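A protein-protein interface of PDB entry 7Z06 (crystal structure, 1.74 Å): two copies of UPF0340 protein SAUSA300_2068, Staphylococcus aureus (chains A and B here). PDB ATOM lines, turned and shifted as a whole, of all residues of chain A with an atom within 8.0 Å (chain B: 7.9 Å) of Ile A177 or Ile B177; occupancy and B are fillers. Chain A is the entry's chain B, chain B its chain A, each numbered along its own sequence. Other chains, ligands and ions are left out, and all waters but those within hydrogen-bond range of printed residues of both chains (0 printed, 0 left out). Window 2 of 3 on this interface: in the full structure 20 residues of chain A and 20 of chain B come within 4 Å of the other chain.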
ATOM      1  N   GLY A  48       9.648 -24.769  -8.358  1.00  0.00           N
ATOM      2  CA  GLY A  48       9.680 -23.448  -7.779  1.00  0.00           C
ATOM      3  C   GLY A  48       9.663 -22.517  -8.976  1.00  0.00           C
ATOM      4  O   GLY A  48      10.483 -22.649  -9.936  1.00  0.00           O
ATOM      5  N   SER A  50       8.911 -18.307 -10.433  1.00  0.00           N
ATOM      6  CA  SER A  50       8.551 -16.896 -10.470  1.00  0.00           C
ATOM      7  C   SER A  50       8.439 -16.536 -11.956  1.00  0.00           C
ATOM      8  O   SER A  50       9.419 -16.371 -12.692  1.00  0.00           O
ATOM      9  CB  SER A  50       9.626 -16.053  -9.778  1.00  0.00           C
ATOM     10  OG  SER A  50       9.534 -14.698 -10.116  1.00  0.00           O
ATOM     11  N   GLU A  53       9.998 -13.345 -13.213  1.00  0.00           N
ATOM     12  CA  GLU A  53      11.403 -13.439 -13.604  1.00  0.00           C
ATOM     13  C   GLU A  53      11.537 -13.895 -15.061  1.00  0.00           C
ATOM     14  O   GLU A  53      12.428 -13.436 -15.766  1.00  0.00           O
ATOM     15  CB  GLU A  53      12.172 -14.380 -12.685  1.00  0.00           C
ATOM     16  CG  GLU A  53      12.455 -13.838 -11.292  1.00  0.00           C
ATOM     17  CD  GLU A  53      13.524 -12.761 -11.304  1.00  0.00           C
ATOM     18  OE1 GLU A  53      14.488 -12.771 -12.125  1.00  0.00           O
ATOM     19  OE2 GLU A  53      13.408 -11.847 -10.475  1.00  0.00           O
ATOM     20  N   VAL A  54      10.653 -14.788 -15.514  1.00  0.00           N
ATOM     21  CA  VAL A  54      10.687 -15.290 -16.889  1.00  0.00           C
ATOM     22  C   VAL A  54      10.534 -14.143 -17.890  1.00  0.00           C
ATOM     23  O   VAL A  54      11.256 -14.067 -18.905  1.00  0.00           O
ATOM     24  CB  VAL A  54       9.626 -16.365 -17.155  1.00  0.00           C
ATOM     25  CG1 VAL A  54       9.558 -16.711 -18.626  1.00  0.00           C
ATOM     26  CG2 VAL A  54       9.934 -17.630 -16.340  1.00  0.00           C
ATOM     27  N   ILE A 148      13.191 -28.274  -9.780  1.00  0.00           N
ATOM     28  CA  ILE A 148      13.557 -27.261 -10.759  1.00  0.00           C
ATOM     29  C   ILE A 148      13.094 -25.913 -10.224  1.00  0.00           C
ATOM     30  O   ILE A 148      11.924 -25.774  -9.872  1.00  0.00           O
ATOM     31  CB  ILE A 148      12.876 -27.532 -12.107  1.00  0.00           C
ATOM     32  CG1 ILE A 148      13.319 -28.875 -12.670  1.00  0.00           C
ATOM     33  CG2 ILE A 148      13.191 -26.418 -13.119  1.00  0.00           C
ATOM     34  CD1 ILE A 148      12.460 -29.369 -13.813  1.00  0.00           C
ATOM     35  N   ASP A 149      14.026 -24.965 -10.091  1.00  0.00           N
ATOM     36  CA  ASP A 149      13.758 -23.624  -9.595  1.00  0.00           C
ATOM     37  C   ASP A 149      13.953 -22.648 -10.796  1.00  0.00           C
ATOM     38  O   ASP A 149      15.054 -22.515 -11.339  1.00  0.00           O
ATOM     39  CB  ASP A 149      14.736 -23.274  -8.501  1.00  0.00           C
ATOM     40  CG  ASP A 149      14.460 -21.916  -7.833  1.00  0.00           C
ATOM     41  OD1 ASP A 149      13.386 -21.275  -8.074  1.00  0.00           O
ATOM     42  OD2 ASP A 149      15.357 -21.476  -7.045  1.00  0.00           O
ATOM     43  N   ILE A 150      12.867 -21.975 -11.178  1.00  0.00           N
ATOM     44  CA  ILE A 150      12.885 -20.961 -12.245  1.00  0.00           C
ATOM     45  C   ILE A 150      12.726 -19.600 -11.583  1.00  0.00           C
ATOM     46  O   ILE A 150      11.678 -19.301 -11.030  1.00  0.00           O
ATOM     47  CB  ILE A 150      11.755 -21.210 -13.259  1.00  0.00           C
ATOM     48  CG1 ILE A 150      11.934 -22.578 -13.921  1.00  0.00           C
ATOM     49  CG2 ILE A 150      11.759 -20.136 -14.348  1.00  0.00           C
ATOM     50  CD1 ILE A 150      10.759 -23.060 -14.730  1.00  0.00           C
ATOM     51  N   GLY A 151      13.810 -18.828 -11.566  1.00  0.00           N
ATOM     52  CA  GLY A 151      13.845 -17.475 -11.065  1.00  0.00           C
ATOM     53  C   GLY A 151      14.245 -17.324  -9.584  1.00  0.00           C
ATOM     54  O   GLY A 151      13.893 -16.344  -8.939  1.00  0.00           O
ATOM     55  N   GLN A 152      15.048 -18.254  -9.084  1.00  0.00           N
ATOM     56  CA  GLN A 152      15.749 -18.097  -7.811  1.00  0.00           C
ATOM     57  C   GLN A 152      14.776 -17.929  -6.606  1.00  0.00           C
ATOM     58  O   GLN A 152      14.998 -17.080  -5.729  1.00  0.00           O
ATOM     59  CB  GLN A 152      16.696 -16.905  -7.853  1.00  0.00           C
ATOM     60  CG  GLN A 152      17.791 -17.015  -8.928  1.00  0.00           C
ATOM     61  CD  GLN A 152      18.570 -15.737  -9.086  1.00  0.00           C
ATOM     62  OE1 GLN A 152      18.138 -14.787  -9.758  1.00  0.00           O
ATOM     63  NE2 GLN A 152      19.744 -15.701  -8.480  1.00  0.00           N
ATOM     64  N   THR A 153      13.685 -18.694  -6.625  1.00  0.00           N
ATOM     65  CA  THR A 153      12.726 -18.702  -5.513  1.00  0.00           C
ATOM     66  C   THR A 153      13.280 -19.501  -4.321  1.00  0.00           C
ATOM     67  O   THR A 153      12.790 -19.329  -3.190  1.00  0.00           O
ATOM     68  CB  THR A 153      11.361 -19.297  -5.921  1.00  0.00           C
ATOM     69  OG1 THR A 153      11.520 -20.664  -6.326  1.00  0.00           O
ATOM     70  CG2 THR A 153      10.748 -18.522  -6.980  1.00  0.00           C
ATOM     71  N   VAL A 170      21.255 -25.322 -20.831  1.00  0.00           N
ATOM     72  CA  VAL A 170      20.224 -24.280 -20.719  1.00  0.00           C
ATOM     73  C   VAL A 170      20.278 -23.627 -19.333  1.00  0.00           C
ATOM     74  O   VAL A 170      20.004 -24.268 -18.357  1.00  0.00           O
ATOM     75  CB  VAL A 170      18.828 -24.834 -21.023  1.00  0.00           C
ATOM     76  CG1 VAL A 170      17.753 -23.748 -20.856  1.00  0.00           C
ATOM     77  CG2 VAL A 170      18.802 -25.334 -22.447  1.00  0.00           C
ATOM     78  N   LYS A 171      20.652 -22.348 -19.284  1.00  0.00           N
ATOM     79  CA  LYS A 171      20.907 -21.634 -18.038  1.00  0.00           C
ATOM     80  C   LYS A 171      19.758 -20.722 -17.608  1.00  0.00           C
ATOM     81  O   LYS A 171      19.723 -20.292 -16.459  1.00  0.00           O
ATOM     82  CB  LYS A 171      22.154 -20.767 -18.189  1.00  0.00           C
ATOM     83  CG  LYS A 171      23.436 -21.497 -18.612  1.00  0.00           C
ATOM     84  CD  LYS A 171      23.878 -22.415 -17.472  1.00  0.00           C
ATOM     85  CE  LYS A 171      25.210 -23.095 -17.779  1.00  0.00           C
ATOM     86  NZ  LYS A 171      26.278 -22.099 -17.924  1.00  0.00           N
ATOM     87  N   GLN A 172      18.843 -20.431 -18.546  1.00  0.00           N
ATOM     88  CA  GLN A 172      17.744 -19.514 -18.298  1.00  0.00           C
ATOM     89  C   GLN A 172      16.486 -19.991 -19.006  1.00  0.00           C
ATOM     90  O   GLN A 172      16.535 -20.653 -20.064  1.00  0.00           O
ATOM     91  CB  GLN A 172      18.101 -18.117 -18.795  1.00  0.00           C
ATOM     92  CG  GLN A 172      19.121 -17.361 -17.968  1.00  0.00           C
ATOM     93  CD  GLN A 172      19.430 -15.966 -18.461  1.00  0.00           C
ATOM     94  OE1 GLN A 172      20.533 -15.486 -18.216  1.00  0.00           O
ATOM     95  NE2 GLN A 172      18.517 -15.324 -19.210  1.00  0.00           N
ATOM     96  N   VAL A 173      15.334 -19.613 -18.445  1.00  0.00           N
ATOM     97  CA  VAL A 173      14.070 -19.757 -19.121  1.00  0.00           C
ATOM     98  C   VAL A 173      13.530 -18.337 -19.238  1.00  0.00           C
ATOM     99  O   VAL A 173      13.224 -17.692 -18.244  1.00  0.00           O
ATOM    100  CB  VAL A 173      13.115 -20.653 -18.351  1.00  0.00           C
ATOM    101  CG1 VAL A 173      11.735 -20.660 -19.024  1.00  0.00           C
ATOM    102  CG2 VAL A 173      13.729 -22.066 -18.201  1.00  0.00           C
ATOM    103  N   GLY A 174      13.496 -17.824 -20.474  1.00  0.00           N
ATOM    104  CA  GLY A 174      13.293 -16.402 -20.711  1.00  0.00           C
ATOM    105  C   GLY A 174      14.427 -15.677 -20.005  1.00  0.00           C
ATOM    106  O   GLY A 174      15.604 -16.000 -20.194  1.00  0.00           O
ATOM    107  N   GLN A 175      14.072 -14.715 -19.150  1.00  0.00           N
ATOM    108  CA  GLN A 175      15.028 -13.964 -18.351  1.00  0.00           C
ATOM    109  C   GLN A 175      15.310 -14.513 -16.955  1.00  0.00           C
ATOM    110  O   GLN A 175      16.039 -13.890 -16.207  1.00  0.00           O
ATOM    111  CB  GLN A 175      14.546 -12.509 -18.263  1.00  0.00           C
ATOM    112  CG  GLN A 175      14.622 -11.817 -19.620  1.00  0.00           C
ATOM    113  CD  GLN A 175      16.041 -11.920 -20.228  1.00  0.00           C
ATOM    114  OE1 GLN A 175      16.251 -12.592 -21.250  1.00  0.00           O
ATOM    115  NE2 GLN A 175      17.030 -11.267 -19.586  1.00  0.00           N
ATOM    116  N   ALA A 176      14.747 -15.676 -16.639  1.00  0.00           N
ATOM    117  CA  ALA A 176      14.856 -16.261 -15.288  1.00  0.00           C
ATOM    118  C   ALA A 176      15.987 -17.266 -15.212  1.00  0.00           C
ATOM    119  O   ALA A 176      16.024 -18.205 -16.010  1.00  0.00           O
ATOM    120  CB  ALA A 176      13.572 -16.963 -14.908  1.00  0.00           C
ATOM    121  N   ILE A 177      16.879 -17.082 -14.233  1.00  0.00           N
ATOM    122  CA  ILE A 177      17.933 -18.053 -13.951  1.00  0.00           C
ATOM    123  C   ILE A 177      17.260 -19.350 -13.522  1.00  0.00           C
ATOM    124  O   ILE A 177      16.320 -19.348 -12.712  1.00  0.00           O
ATOM    125  CB  ILE A 177      18.839 -17.581 -12.796  1.00  0.00           C
ATOM    126  CG1 ILE A 177      19.561 -16.294 -13.086  1.00  0.00           C
ATOM    127  CG2 ILE A 177      19.799 -18.682 -12.337  1.00  0.00           C
ATOM    128  CD1 ILE A 177      20.433 -16.373 -14.313  1.00  0.00           C
ATOM    129  N   VAL A 178      17.735 -20.480 -14.055  1.00  0.00           N
ATOM    130  CA  VAL A 178      17.183 -21.766 -13.678  1.00  0.00           C
ATOM    131  C   VAL A 178      18.229 -22.589 -12.911  1.00  0.00           C
ATOM    132  O   VAL A 178      19.395 -22.595 -13.283  1.00  0.00           O
ATOM    133  CB  VAL A 178      16.567 -22.498 -14.885  1.00  0.00           C
ATOM    134  CG1 VAL A 178      17.649 -22.954 -15.851  1.00  0.00           C
ATOM    135  CG2 VAL A 178      15.731 -23.683 -14.422  1.00  0.00           C
ATOM    136  N   THR A 179      17.780 -23.214 -11.806  1.00  0.00           N
ATOM    137  CA  THR A 179      18.581 -24.101 -10.949  1.00  0.00           C
ATOM    138  C   THR A 179      17.899 -25.457 -10.943  1.00  0.00           C
ATOM    139  O   THR A 179      16.657 -25.534 -10.805  1.00  0.00           O
ATOM    140  CB  THR A 179      18.636 -23.577  -9.503  1.00  0.00           C
ATOM    141  OG1 THR A 179      19.166 -22.249  -9.516  1.00  0.00           O
ATOM    142  CG2 THR A 179      19.530 -24.446  -8.629  1.00  0.00           C
ATOM    143  N   ILE A 180      18.687 -26.521 -11.094  1.00  0.00           N
ATOM    144  CA  ILE A 180      18.162 -27.878 -11.118  1.00  0.00           C
ATOM    145  C   ILE A 180      18.852 -28.648  -9.981  1.00  0.00           C
ATOM    146  O   ILE A 180      20.085 -28.560  -9.828  1.00  0.00           O
ATOM    147  CB  ILE A 180      18.433 -28.588 -12.469  1.00  0.00           C
ATOM    148  CG1 ILE A 180      18.008 -27.762 -13.698  1.00  0.00           C
ATOM    149  CG2 ILE A 180      17.745 -29.949 -12.498  1.00  0.00           C
ATOM    150  CD1 ILE A 180      16.507 -27.564 -13.808  1.00  0.00           C
ATOM    151  N   GLY B  48      27.235 -20.242   1.498  1.00  0.00           N
ATOM    152  CA  GLY B  48      27.428 -21.224   0.468  1.00  0.00           C
ATOM    153  C   GLY B  48      28.302 -20.536  -0.578  1.00  0.00           C
ATOM    154  O   GLY B  48      27.991 -19.433  -1.034  1.00  0.00           O
ATOM    155  N   SER B  50      31.116 -21.116  -4.103  1.00  0.00           N
ATOM    156  CA  SER B  50      31.919 -21.770  -5.128  1.00  0.00           C
ATOM    157  C   SER B  50      32.872 -20.720  -5.693  1.00  0.00           C
ATOM    158  O   SER B  50      32.443 -19.821  -6.432  1.00  0.00           O
ATOM    159  CB  SER B  50      31.013 -22.363  -6.206  1.00  0.00           C
ATOM    160  OG  SER B  50      31.732 -22.680  -7.383  1.00  0.00           O
ATOM    161  N   GLU B  53      33.114 -20.341  -9.443  1.00  0.00           N
ATOM    162  CA  GLU B  53      32.073 -19.520 -10.055  1.00  0.00           C
ATOM    163  C   GLU B  53      32.453 -18.044 -10.039  1.00  0.00           C
ATOM    164  O   GLU B  53      32.145 -17.324 -10.984  1.00  0.00           O
ATOM    165  CB  GLU B  53      30.724 -19.741  -9.371  1.00  0.00           C
ATOM    166  CG  GLU B  53      30.044 -21.076  -9.706  1.00  0.00           C
ATOM    167  CD  GLU B  53      29.517 -21.104 -11.142  1.00  0.00           C
ATOM    168  OE1 GLU B  53      28.948 -20.080 -11.589  1.00  0.00           O
ATOM    169  OE2 GLU B  53      29.671 -22.128 -11.865  1.00  0.00           O
ATOM    170  N   VAL B  54      33.117 -17.596  -8.964  1.00  0.00           N
ATOM    171  CA  VAL B  54      33.528 -16.198  -8.843  1.00  0.00           C
ATOM    172  C   VAL B  54      34.469 -15.805  -9.986  1.00  0.00           C
ATOM    173  O   VAL B  54      34.336 -14.732 -10.578  1.00  0.00           O
ATOM    174  CB  VAL B  54      34.187 -15.900  -7.478  1.00  0.00           C
ATOM    175  CG1 VAL B  54      34.840 -14.505  -7.489  1.00  0.00           C
ATOM    176  CG2 VAL B  54      33.129 -15.989  -6.370  1.00  0.00           C
ATOM    177  N   ILE B 148      23.751 -16.517   2.536  1.00  0.00           N
ATOM    178  CA  ILE B 148      24.218 -15.941   1.268  1.00  0.00           C
ATOM    179  C   ILE B 148      24.810 -17.095   0.468  1.00  0.00           C
ATOM    180  O   ILE B 148      25.690 -17.822   0.974  1.00  0.00           O
ATOM    181  CB  ILE B 148      25.308 -14.891   1.513  1.00  0.00           C
ATOM    182  CG1 ILE B 148      24.753 -13.754   2.372  1.00  0.00           C
ATOM    183  CG2 ILE B 148      25.871 -14.367   0.210  1.00  0.00           C
ATOM    184  CD1 ILE B 148      25.806 -12.765   2.860  1.00  0.00           C
ATOM    185  N   ASP B 149      24.294 -17.282  -0.754  1.00  0.00           N
ATOM    186  CA  ASP B 149      24.778 -18.285  -1.681  1.00  0.00           C
ATOM    187  C   ASP B 149      25.504 -17.583  -2.847  1.00  0.00           C
ATOM    188  O   ASP B 149      24.890 -16.806  -3.591  1.00  0.00           O
ATOM    189  CB  ASP B 149      23.575 -19.068  -2.198  1.00  0.00           C
ATOM    190  CG  ASP B 149      23.961 -20.252  -3.077  1.00  0.00           C
ATOM    191  OD1 ASP B 149      25.199 -20.619  -3.174  1.00  0.00           O
ATOM    192  OD2 ASP B 149      23.009 -20.822  -3.706  1.00  0.00           O
ATOM    193  N   ILE B 150      26.802 -17.862  -2.985  1.00  0.00           N
ATOM    194  CA  ILE B 150      27.633 -17.303  -4.079  1.00  0.00           C
ATOM    195  C   ILE B 150      27.939 -18.457  -5.024  1.00  0.00           C
ATOM    196  O   ILE B 150      28.681 -19.407  -4.670  1.00  0.00           O
ATOM    197  CB  ILE B 150      28.938 -16.699  -3.528  1.00  0.00           C
ATOM    198  CG1 ILE B 150      28.603 -15.551  -2.568  1.00  0.00           C
ATOM    199  CG2 ILE B 150      29.851 -16.208  -4.629  1.00  0.00           C
ATOM    200  CD1 ILE B 150      29.720 -15.057  -1.702  1.00  0.00           C
ATOM    201  N   GLY B 151      27.303 -18.425  -6.191  1.00  0.00           N
ATOM    202  CA  GLY B 151      27.514 -19.398  -7.233  1.00  0.00           C
ATOM    203  C   GLY B 151      26.553 -20.588  -7.247  1.00  0.00           C
ATOM    204  O   GLY B 151      26.876 -21.630  -7.791  1.00  0.00           O
ATOM    205  N   GLN B 152      25.339 -20.396  -6.730  1.00  0.00           N
ATOM    206  CA  GLN B 152      24.240 -21.336  -6.944  1.00  0.00           C
ATOM    207  C   GLN B 152      24.537 -22.754  -6.369  1.00  0.00           C
ATOM    208  O   GLN B 152      24.223 -23.753  -6.998  1.00  0.00           O
ATOM    209  CB  GLN B 152      23.892 -21.444  -8.416  1.00  0.00           C
ATOM    210  CG  GLN B 152      23.423 -20.119  -9.029  1.00  0.00           C
ATOM    211  CD  GLN B 152      23.239 -20.213 -10.536  1.00  0.00           C
ATOM    212  OE1 GLN B 152      22.237 -20.730 -11.029  1.00  0.00           O
ATOM    213  NE2 GLN B 152      24.218 -19.730 -11.274  1.00  0.00           N
ATOM    214  N   THR B 153      25.180 -22.784  -5.200  1.00  0.00           N
ATOM    215  CA  THR B 153      25.474 -24.043  -4.494  1.00  0.00           C
ATOM    216  C   THR B 153      24.235 -24.596  -3.817  1.00  0.00           C
ATOM    217  O   THR B 153      24.186 -25.796  -3.500  1.00  0.00           O
ATOM    218  CB  THR B 153      26.598 -23.867  -3.440  1.00  0.00           C
ATOM    219  OG1 THR B 153      26.170 -22.934  -2.436  1.00  0.00           O
ATOM    220  CG2 THR B 153      27.879 -23.373  -4.102  1.00  0.00           C
ATOM    221  N   VAL B 170      23.219  -5.555  -6.109  1.00  0.00           N
ATOM    222  CA  VAL B 170      24.367  -6.394  -6.492  1.00  0.00           C
ATOM    223  C   VAL B 170      23.908  -7.822  -6.798  1.00  0.00           C
ATOM    224  O   VAL B 170      23.439  -8.510  -5.918  1.00  0.00           O
ATOM    225  CB  VAL B 170      25.458  -6.374  -5.415  1.00  0.00           C
ATOM    226  CG1 VAL B 170      26.624  -7.289  -5.802  1.00  0.00           C
ATOM    227  CG2 VAL B 170      25.983  -4.960  -5.230  1.00  0.00           C
ATOM    228  N   LYS B 171      24.035  -8.232  -8.066  1.00  0.00           N
ATOM    229  CA  LYS B 171      23.487  -9.513  -8.535  1.00  0.00           C
ATOM    230  C   LYS B 171      24.552 -10.612  -8.671  1.00  0.00           C
ATOM    231  O   LYS B 171      24.221 -11.771  -8.783  1.00  0.00           O
ATOM    232  CB  LYS B 171      22.827  -9.339  -9.893  1.00  0.00           C
ATOM    233  CG  LYS B 171      21.803  -8.221 -10.024  1.00  0.00           C
ATOM    234  CD  LYS B 171      20.559  -8.549  -9.256  1.00  0.00           C
ATOM    235  CE  LYS B 171      19.488  -7.458  -9.426  1.00  0.00           C
ATOM    236  NZ  LYS B 171      18.358  -7.853  -8.519  1.00  0.00           N
ATOM    237  N   GLN B 172      25.826 -10.211  -8.679  1.00  0.00           N
ATOM    238  CA  GLN B 172      26.944 -11.115  -8.889  1.00  0.00           C
ATOM    239  C   GLN B 172      28.125 -10.698  -8.042  1.00  0.00           C
ATOM    240  O   GLN B 172      28.329  -9.516  -7.753  1.00  0.00           O
ATOM    241  CB  GLN B 172      27.366 -11.150 -10.369  1.00  0.00           C
ATOM    242  CG  GLN B 172      26.413 -11.833 -11.309  1.00  0.00           C
ATOM    243  CD  GLN B 172      26.870 -11.828 -12.751  1.00  0.00           C
ATOM    244  OE1 GLN B 172      27.993 -11.444 -13.100  1.00  0.00           O
ATOM    245  NE2 GLN B 172      25.972 -12.240 -13.621  1.00  0.00           N
ATOM    246  N   VAL B 173      28.936 -11.695  -7.674  1.00  0.00           N
ATOM    247  CA  VAL B 173      30.227 -11.473  -7.088  1.00  0.00           C
ATOM    248  C   VAL B 173      31.220 -12.084  -8.065  1.00  0.00           C
ATOM    249  O   VAL B 173      31.246 -13.292  -8.255  1.00  0.00           O
ATOM    250  CB  VAL B 173      30.320 -12.078  -5.700  1.00  0.00           C
ATOM    251  CG1 VAL B 173      31.750 -12.021  -5.182  1.00  0.00           C
ATOM    252  CG2 VAL B 173      29.352 -11.341  -4.770  1.00  0.00           C
ATOM    253  N   GLY B 174      31.984 -11.223  -8.741  1.00  0.00           N
ATOM    254  CA  GLY B 174      32.721 -11.613  -9.938  1.00  0.00           C
ATOM    255  C   GLY B 174      31.720 -12.146 -10.944  1.00  0.00           C
ATOM    256  O   GLY B 174      30.774 -11.470 -11.262  1.00  0.00           O
ATOM    257  N   GLN B 175      31.925 -13.381 -11.407  1.00  0.00           N
ATOM    258  CA  GLN B 175      31.021 -14.043 -12.341  1.00  0.00           C
ATOM    259  C   GLN B 175      29.956 -14.932 -11.678  1.00  0.00           C
ATOM    260  O   GLN B 175      29.197 -15.591 -12.379  1.00  0.00           O
ATOM    261  CB  GLN B 175      31.838 -14.890 -13.307  1.00  0.00           C
ATOM    262  CG  GLN B 175      32.769 -14.082 -14.165  1.00  0.00           C
ATOM    263  CD  GLN B 175      32.061 -12.984 -14.934  1.00  0.00           C
ATOM    264  OE1 GLN B 175      32.299 -11.805 -14.689  1.00  0.00           O
ATOM    265  NE2 GLN B 175      31.193 -13.359 -15.875  1.00  0.00           N
ATOM    266  N   ALA B 176      29.916 -14.954 -10.339  1.00  0.00           N
ATOM    267  CA  ALA B 176      29.024 -15.858  -9.594  1.00  0.00           C
ATOM    268  C   ALA B 176      27.726 -15.212  -9.232  1.00  0.00           C
ATOM    269  O   ALA B 176      27.728 -14.150  -8.616  1.00  0.00           O
ATOM    270  CB  ALA B 176      29.688 -16.347  -8.325  1.00  0.00           C
ATOM    271  N   ILE B 177      26.612 -15.849  -9.624  1.00  0.00           N
ATOM    272  CA  ILE B 177      25.284 -15.376  -9.291  1.00  0.00           C
ATOM    273  C   ILE B 177      25.150 -15.464  -7.779  1.00  0.00           C
ATOM    274  O   ILE B 177      25.545 -16.460  -7.174  1.00  0.00           O
ATOM    275  CB  ILE B 177      24.195 -16.206  -9.974  1.00  0.00           C
ATOM    276  CG1 ILE B 177      24.233 -15.906 -11.474  1.00  0.00           C
ATOM    277  CG2 ILE B 177      22.804 -15.930  -9.366  1.00  0.00           C
ATOM    278  CD1 ILE B 177      23.311 -16.745 -12.319  1.00  0.00           C
ATOM    279  N   VAL B 178      24.606 -14.408  -7.172  1.00  0.00           N
ATOM    280  CA  VAL B 178      24.455 -14.404  -5.716  1.00  0.00           C
ATOM    281  C   VAL B 178      22.972 -14.399  -5.363  1.00  0.00           C
ATOM    282  O   VAL B 178      22.186 -13.684  -5.994  1.00  0.00           O
ATOM    283  CB  VAL B 178      25.270 -13.269  -5.057  1.00  0.00           C
ATOM    284  CG1 VAL B 178      24.690 -11.918  -5.387  1.00  0.00           C
ATOM    285  CG2 VAL B 178      25.347 -13.489  -3.573  1.00  0.00           C
ATOM    286  N   THR B 179      22.612 -15.262  -4.397  1.00  0.00           N
ATOM    287  CA  THR B 179      21.251 -15.381  -3.835  1.00  0.00           C
ATOM    288  C   THR B 179      21.340 -15.121  -2.344  1.00  0.00           C
ATOM    289  O   THR B 179      22.268 -15.598  -1.692  1.00  0.00           O
ATOM    290  CB  THR B 179      20.684 -16.804  -4.059  1.00  0.00           C
ATOM    291  OG1 THR B 179      20.563 -16.979  -5.484  1.00  0.00           O
ATOM    292  CG2 THR B 179      19.272 -16.900  -3.601  1.00  0.00           C
ATOM    293  N   ILE B 180      20.403 -14.341  -1.797  1.00  0.00           N
ATOM    294  CA  ILE B 180      20.412 -13.975  -0.389  1.00  0.00           C
ATOM    295  C   ILE B 180      19.067 -14.418   0.199  1.00  0.00           C
ATOM    296  O   ILE B 180      18.020 -14.153  -0.400  1.00  0.00           O
ATOM    297  CB  ILE B 180      20.586 -12.433  -0.184  1.00  0.00           C
ATOM    298  CG1 ILE B 180      21.739 -11.824  -0.984  1.00  0.00           C
ATOM    299  CG2 ILE B 180      20.705 -12.096   1.294  1.00  0.00           C
ATOM    300  CD1 ILE B 180      23.082 -12.271  -0.501  1.00  0.00           C
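Hydrophobic or aromatic side chains of chain B within 4 Å of the printed part of chain A: Ile B177.
Among the printed residues, no Asp or Glu carboxylate lies within 4 Å of a Lys or Arg side-chain nitrogen of the other chain.
The side-chain hydroxyl (OG1) of Thr B179 lies within hydrogen-bond range of the side-chain amide nitrogen (NE2) of Gln A152 (3.4 Å).
Among the printed residues, merely in contact across the chains: Gln A152 with Ile B177 (3.2 Å), Ile A177 with Gln B152 (3.4 Å), Ile A177 with Ile B177 (3.5 Å) and Thr A179 with Gln B152 (3.7 Å).
The backbone carbonyl oxygen (O) of Thr B179 sits at hydrogen-bond distance from the backbone NH (N) of Asp B149 (2.8 Å).
The backbone NH of Asp A149 is in hydrogen-bond range of the backbone carbonyl oxygen of Thr A179.
The backbone carbonyl oxygen (O) of Ile B177 is in hydrogen-bond range of the backbone NH (N) of Gly B151.
N of Gly A151 sits at hydrogen-bond distance from O of Ile A177 (2.8 Å).
Of the printed residues of chain A, Ile B177 touches Gln A152 (3.2 Å) and Ile A177 (3.5 Å).
No residue of chain B comes within 4 Å of Ala A176.
No residue of chain A comes within 4 Å of Ala B176.
Of the printed residues of chain A, Thr B179 touches Gln A152 (3.4 Å).
Of the printed residues of chain B, Gln A152 touches Ile B177 and Thr B179.
Gly A151 touches none of the printed residues of chain B.
Gln A152 touches Ile B177, and with the chains exchanged Ile A177 touches Gln B152.
Gln A152 touches Thr B179, and with the chains exchanged Thr A179 touches Gln B152.
Ile A177 touches its own counterpart, Ile B177.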
